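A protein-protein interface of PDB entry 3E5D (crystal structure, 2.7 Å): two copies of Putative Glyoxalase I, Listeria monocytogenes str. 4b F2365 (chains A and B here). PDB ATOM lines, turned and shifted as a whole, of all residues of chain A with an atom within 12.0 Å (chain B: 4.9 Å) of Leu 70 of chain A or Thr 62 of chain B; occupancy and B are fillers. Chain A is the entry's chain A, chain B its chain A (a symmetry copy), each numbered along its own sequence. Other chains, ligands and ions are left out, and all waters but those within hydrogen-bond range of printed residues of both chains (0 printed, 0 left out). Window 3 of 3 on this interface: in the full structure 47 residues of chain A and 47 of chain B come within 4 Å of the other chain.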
ATOM      1  N   LYS A  64      -7.507 -17.915  18.686  1.00  0.00           N
ATOM      2  CA  LYS A  64      -6.111 -18.316  18.409  1.00  0.00           C
ATOM      3  C   LYS A  64      -5.262 -18.057  19.685  1.00  0.00           C
ATOM      4  O   LYS A  64      -5.508 -17.086  20.409  1.00  0.00           O
ATOM      5  CB  LYS A  64      -5.527 -17.521  17.212  1.00  0.00           C
ATOM      6  CG  LYS A  64      -6.276 -17.624  15.871  1.00  0.00           C
ATOM      7  N   THR A  65      -4.285 -18.927  19.965  1.00  0.00           N
ATOM      8  CA  THR A  65      -3.389 -18.769  21.128  1.00  0.00           C
ATOM      9  C   THR A  65      -2.074 -18.089  20.689  1.00  0.00           C
ATOM     10  O   THR A  65      -1.454 -18.500  19.704  1.00  0.00           O
ATOM     11  CB  THR A  65      -3.095 -20.130  21.821  1.00  0.00           C
ATOM     12  OG1 THR A  65      -2.391 -20.994  20.918  1.00  0.00           O
ATOM     13  CG2 THR A  65      -4.397 -20.806  22.285  1.00  0.00           C
ATOM     14  N   THR A  66      -1.644 -17.075  21.448  1.00  0.00           N
ATOM     15  CA  THR A  66      -0.469 -16.241  21.095  1.00  0.00           C
ATOM     16  C   THR A  66       0.884 -16.979  20.881  1.00  0.00           C
ATOM     17  O   THR A  66       1.340 -17.063  19.740  1.00  0.00           O
ATOM     18  CB  THR A  66      -0.291 -14.994  22.073  1.00  0.00           C
ATOM     19  OG1 THR A  66       0.054 -15.435  23.391  1.00  0.00           O
ATOM     20  CG2 THR A  66      -1.572 -14.104  22.140  1.00  0.00           C
ATOM     21  N   GLY A  67       1.515 -17.524  21.926  1.00  0.00           N
ATOM     22  CA  GLY A  67       2.860 -18.134  21.763  1.00  0.00           C
ATOM     23  C   GLY A  67       3.026 -19.599  22.142  1.00  0.00           C
ATOM     24  O   GLY A  67       2.408 -20.466  21.520  1.00  0.00           O
ATOM     25  N   GLU A  68       3.926 -19.874  23.101  1.00  0.00           N
ATOM     26  CA  GLU A  68       4.140 -21.227  23.676  1.00  0.00           C
ATOM     27  C   GLU A  68       3.633 -21.205  25.124  1.00  0.00           C
ATOM     28  O   GLU A  68       4.198 -20.545  25.989  1.00  0.00           O
ATOM     29  CB  GLU A  68       5.592 -21.702  23.584  1.00  0.00           C
ATOM     30  CG  GLU A  68       5.917 -22.337  22.233  1.00  0.00           C
ATOM     31  CD  GLU A  68       7.295 -23.021  22.180  1.00  0.00           C
ATOM     32  OE1 GLU A  68       8.285 -22.448  22.708  1.00  0.00           O
ATOM     33  OE2 GLU A  68       7.385 -24.127  21.583  1.00  0.00           O
ATOM     34  N   ASN A  69       2.554 -21.951  25.354  1.00  0.00           N
ATOM     35  CA  ASN A  69       1.813 -21.941  26.607  1.00  0.00           C
ATOM     36  C   ASN A  69       1.587 -23.316  27.228  1.00  0.00           C
ATOM     37  O   ASN A  69       1.742 -24.348  26.554  1.00  0.00           O
ATOM     38  CB  ASN A  69       0.438 -21.347  26.304  1.00  0.00           C
ATOM     39  CG  ASN A  69       0.522 -19.972  25.692  1.00  0.00           C
ATOM     40  OD1 ASN A  69       1.061 -19.049  26.299  1.00  0.00           O
ATOM     41  ND2 ASN A  69      -0.030 -19.821  24.492  1.00  0.00           N
ATOM     42  N   LEU A  70       1.192 -23.309  28.508  1.00  0.00           N
ATOM     43  CA  LEU A  70       0.853 -24.535  29.231  1.00  0.00           C
ATOM     44  C   LEU A  70      -0.292 -25.203  28.472  1.00  0.00           C
ATOM     45  O   LEU A  70      -1.208 -24.530  28.007  1.00  0.00           O
ATOM     46  CB  LEU A  70       0.444 -24.237  30.680  1.00  0.00           C
ATOM     47  CG  LEU A  70       1.504 -23.642  31.622  1.00  0.00           C
ATOM     48  CD1 LEU A  70       0.923 -23.311  33.000  1.00  0.00           C
ATOM     49  CD2 LEU A  70       2.696 -24.572  31.768  1.00  0.00           C
ATOM     50  N   GLY A  71      -0.219 -26.518  28.315  1.00  0.00           N
ATOM     51  CA  GLY A  71      -1.241 -27.270  27.591  1.00  0.00           C
ATOM     52  C   GLY A  71      -0.596 -28.102  26.512  1.00  0.00           C
ATOM     53  O   GLY A  71       0.628 -28.224  26.476  1.00  0.00           O
ATOM     54  N   TRP A  72      -1.404 -28.653  25.611  1.00  0.00           N
ATOM     55  CA  TRP A  72      -0.871 -29.514  24.554  1.00  0.00           C
ATOM     56  C   TRP A  72       0.117 -28.744  23.686  1.00  0.00           C
ATOM     57  O   TRP A  72      -0.209 -27.685  23.197  1.00  0.00           O
ATOM     58  CB  TRP A  72      -2.012 -30.119  23.748  1.00  0.00           C
ATOM     59  CG  TRP A  72      -2.912 -30.906  24.626  1.00  0.00           C
ATOM     60  CD1 TRP A  72      -4.178 -30.591  24.981  1.00  0.00           C
ATOM     61  CD2 TRP A  72      -2.583 -32.113  25.328  1.00  0.00           C
ATOM     62  NE1 TRP A  72      -4.684 -31.542  25.838  1.00  0.00           N
ATOM     63  CE2 TRP A  72      -3.723 -32.486  26.071  1.00  0.00           C
ATOM     64  CE3 TRP A  72      -1.441 -32.926  25.385  1.00  0.00           C
ATOM     65  CZ2 TRP A  72      -3.759 -33.635  26.868  1.00  0.00           C
ATOM     66  CZ3 TRP A  72      -1.474 -34.071  26.180  1.00  0.00           C
ATOM     67  CH2 TRP A  72      -2.627 -34.415  26.909  1.00  0.00           C
ATOM     68  N   ALA A  73       1.323 -29.287  23.511  1.00  0.00           N
ATOM     69  CA  ALA A  73       2.428 -28.587  22.826  1.00  0.00           C
ATOM     70  C   ALA A  73       2.614 -28.884  21.336  1.00  0.00           C
ATOM     71  O   ALA A  73       2.707 -27.958  20.530  1.00  0.00           O
ATOM     72  CB  ALA A  73       3.733 -28.868  23.558  1.00  0.00           C
ATOM     73  N   HIS A  74       2.730 -30.159  20.980  1.00  0.00           N
ATOM     74  CA  HIS A  74       2.939 -30.549  19.589  1.00  0.00           C
ATOM     75  C   HIS A  74       2.715 -32.037  19.420  1.00  0.00           C
ATOM     76  O   HIS A  74       2.360 -32.734  20.364  1.00  0.00           O
ATOM     77  CB  HIS A  74       4.379 -30.202  19.151  1.00  0.00           C
ATOM     78  CG  HIS A  74       5.459 -30.946  19.895  1.00  0.00           C
ATOM     79  ND1 HIS A  74       6.195 -30.373  20.912  1.00  0.00           N
ATOM     80  CD2 HIS A  74       5.938 -32.210  19.752  1.00  0.00           C
ATOM     81  CE1 HIS A  74       7.070 -31.257  21.368  1.00  0.00           C
ATOM     82  NE2 HIS A  74       6.934 -32.381  20.683  1.00  0.00           N
ATOM     83  N   ARG A 122       2.607 -26.776  15.716  1.00  0.00           N
ATOM     84  CA  ARG A 122       3.941 -27.400  15.665  1.00  0.00           C
ATOM     85  C   ARG A 122       3.895 -28.894  15.440  1.00  0.00           C
ATOM     86  O   ARG A 122       3.121 -29.591  16.071  1.00  0.00           O
ATOM     87  CB  ARG A 122       4.716 -27.149  16.960  1.00  0.00           C
ATOM     88  CG  ARG A 122       5.009 -25.680  17.221  1.00  0.00           C
ATOM     89  CD  ARG A 122       5.646 -25.460  18.585  1.00  0.00           C
ATOM     90  NE  ARG A 122       6.835 -26.301  18.760  1.00  0.00           N
ATOM     91  CZ  ARG A 122       8.074 -25.947  18.422  1.00  0.00           C
ATOM     92  NH1 ARG A 122       8.325 -24.754  17.880  1.00  0.00           N
ATOM     93  NH2 ARG A 122       9.072 -26.799  18.629  1.00  0.00           N
ATOM     94  N   TRP B  10       3.033 -29.127  27.616  1.00  0.00           N
ATOM     95  CA  TRP B  10       3.720 -28.145  28.464  1.00  0.00           C
ATOM     96  C   TRP B  10       3.087 -28.177  29.842  1.00  0.00           C
ATOM     97  O   TRP B  10       1.876 -28.019  30.005  1.00  0.00           O
ATOM     98  CB  TRP B  10       3.697 -26.717  27.908  1.00  0.00           C
ATOM     99  CG  TRP B  10       4.744 -26.440  26.877  1.00  0.00           C
ATOM    100  CD1 TRP B  10       4.539 -26.056  25.593  1.00  0.00           C
ATOM    101  CD2 TRP B  10       6.163 -26.540  27.044  1.00  0.00           C
ATOM    102  NE1 TRP B  10       5.739 -25.891  24.946  1.00  0.00           N
ATOM    103  CE2 TRP B  10       6.754 -26.192  25.814  1.00  0.00           C
ATOM    104  CE3 TRP B  10       6.993 -26.893  28.112  1.00  0.00           C
ATOM    105  CZ2 TRP B  10       8.133 -26.186  25.619  1.00  0.00           C
ATOM    106  CZ3 TRP B  10       8.363 -26.881  27.916  1.00  0.00           C
ATOM    107  CH2 TRP B  10       8.918 -26.525  26.679  1.00  0.00           C
ATOM    108  N   THR B  11       3.938 -28.361  30.835  1.00  0.00           N
ATOM    109  CA  THR B  11       3.495 -28.531  32.184  1.00  0.00           C
ATOM    110  C   THR B  11       4.175 -27.565  33.150  1.00  0.00           C
ATOM    111  O   THR B  11       5.313 -27.133  32.947  1.00  0.00           O
ATOM    112  CB  THR B  11       3.775 -29.970  32.631  1.00  0.00           C
ATOM    113  OG1 THR B  11       2.979 -30.248  33.772  1.00  0.00           O
ATOM    114  CG2 THR B  11       5.259 -30.178  32.982  1.00  0.00           C
ATOM    115  N   THR B  12       3.458 -27.225  34.208  1.00  0.00           N
ATOM    116  CA  THR B  12       3.986 -26.340  35.231  1.00  0.00           C
ATOM    117  C   THR B  12       4.573 -27.151  36.404  1.00  0.00           C
ATOM    118  O   THR B  12       5.605 -26.789  36.933  1.00  0.00           O
ATOM    119  CB  THR B  12       2.978 -25.220  35.659  1.00  0.00           C
ATOM    120  OG1 THR B  12       3.233 -24.904  37.010  1.00  0.00           O
ATOM    121  CG2 THR B  12       1.515 -25.633  35.572  1.00  0.00           C
ATOM    122  N   THR B  59      11.145 -22.967  32.679  1.00  0.00           N
ATOM    123  CA  THR B  59      10.926 -21.744  33.430  1.00  0.00           C
ATOM    124  C   THR B  59      10.243 -20.623  32.624  1.00  0.00           C
ATOM    125  O   THR B  59       9.422 -19.914  33.190  1.00  0.00           O
ATOM    126  CB  THR B  59      12.222 -21.314  34.189  1.00  0.00           C
ATOM    127  OG1 THR B  59      13.338 -21.409  33.306  1.00  0.00           O
ATOM    128  CG2 THR B  59      12.482 -22.253  35.394  1.00  0.00           C
ATOM    129  N   ASP B  60      10.500 -20.498  31.315  1.00  0.00           N
ATOM    130  CA  ASP B  60       9.804 -19.452  30.526  1.00  0.00           C
ATOM    131  C   ASP B  60       8.373 -19.815  30.025  1.00  0.00           C
ATOM    132  O   ASP B  60       7.576 -18.911  29.768  1.00  0.00           O
ATOM    133  CB  ASP B  60      10.673 -18.904  29.383  1.00  0.00           C
ATOM    134  CG  ASP B  60      10.804 -19.849  28.222  1.00  0.00           C
ATOM    135  OD1 ASP B  60       9.868 -20.617  27.927  1.00  0.00           O
ATOM    136  OD2 ASP B  60      11.858 -19.794  27.566  1.00  0.00           O
ATOM    137  N   VAL B  61       8.050 -21.106  29.872  1.00  0.00           N
ATOM    138  CA  VAL B  61       6.697 -21.511  29.424  1.00  0.00           C
ATOM    139  C   VAL B  61       5.754 -21.417  30.618  1.00  0.00           C
ATOM    140  O   VAL B  61       5.675 -22.310  31.453  1.00  0.00           O
ATOM    141  CB  VAL B  61       6.660 -22.900  28.784  1.00  0.00           C
ATOM    142  CG1 VAL B  61       5.214 -23.313  28.506  1.00  0.00           C
ATOM    143  CG2 VAL B  61       7.508 -22.909  27.494  1.00  0.00           C
ATOM    144  N   THR B  62       4.995 -20.332  30.632  1.00  0.00           N
ATOM    145  CA  THR B  62       4.236 -19.943  31.796  1.00  0.00           C
ATOM    146  C   THR B  62       2.738 -19.628  31.627  1.00  0.00           C
ATOM    147  O   THR B  62       1.966 -19.807  32.572  1.00  0.00           O
ATOM    148  CB  THR B  62       4.943 -18.697  32.366  1.00  0.00           C
ATOM    149  OG1 THR B  62       4.214 -18.219  33.484  1.00  0.00           O
ATOM    150  CG2 THR B  62       5.056 -17.572  31.313  1.00  0.00           C
ATOM    151  N   GLY B  63       2.330 -19.169  30.443  1.00  0.00           N
ATOM    152  CA  GLY B  63       0.940 -18.757  30.191  1.00  0.00           C
ATOM    153  C   GLY B  63      -0.113 -19.848  30.110  1.00  0.00           C
ATOM    154  O   GLY B  63       0.152 -20.919  29.587  1.00  0.00           O
ATOM    155  N   LYS B  64      -1.308 -19.562  30.643  1.00  0.00           N
ATOM    156  CA  LYS B  64      -2.468 -20.479  30.617  1.00  0.00           C
ATOM    157  C   LYS B  64      -3.450 -19.999  29.511  1.00  0.00           C
ATOM    158  O   LYS B  64      -3.594 -18.792  29.290  1.00  0.00           O
ATOM    159  CB  LYS B  64      -3.189 -20.511  31.990  1.00  0.00           C
ATOM    160  CG  LYS B  64      -2.348 -20.921  33.213  1.00  0.00           C
ATOM    161  N   THR B  65      -4.103 -20.936  28.814  1.00  0.00           N
ATOM    162  CA  THR B  65      -5.086 -20.605  27.764  1.00  0.00           C
ATOM    163  C   THR B  65      -6.515 -20.653  28.349  1.00  0.00           C
ATOM    164  O   THR B  65      -6.887 -21.623  29.016  1.00  0.00           O
ATOM    165  CB  THR B  65      -4.966 -21.554  26.539  1.00  0.00           C
ATOM    166  OG1 THR B  65      -5.273 -22.899  26.932  1.00  0.00           O
ATOM    167  CG2 THR B  65      -3.553 -21.496  25.932  1.00  0.00           C
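Thr 65 of chain A touches its own counterpart, Thr 65 of chain B. Of the 13 pairs that touch across the chains among the printed residues, 1 has its exchanged pair printed and touching as well.
The side-chain carboxylate of Glu 68 of chain A lies within salt-bridge range of the guanidinium group of Arg 122 of chain A (3.6 Å).
Thr 65 of chain A touches Thr 65 of chain B. Glu 68 of chain A touches Val 61 of chain B (O to CG1, 3.9 Å). O of Asn 69 of chain A touches CB of Trp 10 of chain B (3.4 Å). Asn 69 of chain A touches Val 61 of chain B (C to CG1, 3.8 Å). Gly 63 of chain B touches Asn 69 of chain A. C of Thr 11 of chain B touches CD2 of Leu 70 of chain A, at 3.6 Å. Leu 70 of chain A touches Thr 12 of chain B. Val 61 of chain B touches Leu 70 of chain A. CD1 of Leu 70 of chain A touches O of Thr 62 of chain B, 3.7 Å away. CB of Ala 73 of chain A touches CD1 of Trp 10 of chain B, 3.6 Å away.
N of Trp 10 of chain B lies within hydrogen-bond range of O of Gly 71 of chain A (2.8 Å). The backbone NH (N) of Leu 70 of chain A lies within hydrogen-bond range of the backbone carbonyl oxygen (O) of Gly 63 of chain B (2.8 Å).
Lys 64 of chain A touches none of the printed residues of chain B. Of the printed residues of chain B, Thr 65 of chain A touches Thr 65 (3.8 Å). Leu 70 of chain A touches six residues of chain B. Of the printed residues of chain A, Trp 10 of chain B touches Asn 69, Leu 70, Gly 71 and Ala 73. Thr 59 of chain B touches none of the printed residues of chain A. No residue of chain A comes within 4 Å of Asp 60 of chain B. Thr 62 of chain B touches one residue of chain A. Gly 63 of chain B touches just these residues of chain A: Asn 69 and Leu 70. Lys 64 of chain B touches none of the printed residues of chain A. Printed residues of chain A within 4 Å of Thr 65 of chain B: Thr 65. The nearest residue of chain B that does not touch Leu 70 of chain A is Lys 64 of chain B (4.1 Å).
Of the 12 printed residues of chain A, 6 touch a printed residue of chain B. Hydrophobic or aromatic side chains of chain A within 4 Å of the printed part of chain B: Leu 70 and Ala 73. Printed residues of chain B that touch a printed residue of chain A: Trp 10, Thr 11, Thr 12, Val 61, Thr 62, Gly 63 and Thr 65. Hydrophobic or aromatic side chains of chain B within 4 Å of the printed part of chain A: Trp 10 and Val 61. Among the printed residues, 13 pairs touch across the chains. Among the printed residues, no Asp or Glu carboxylate lies within 4 Å of a Lys or Arg side-chain nitrogen of the other chain.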
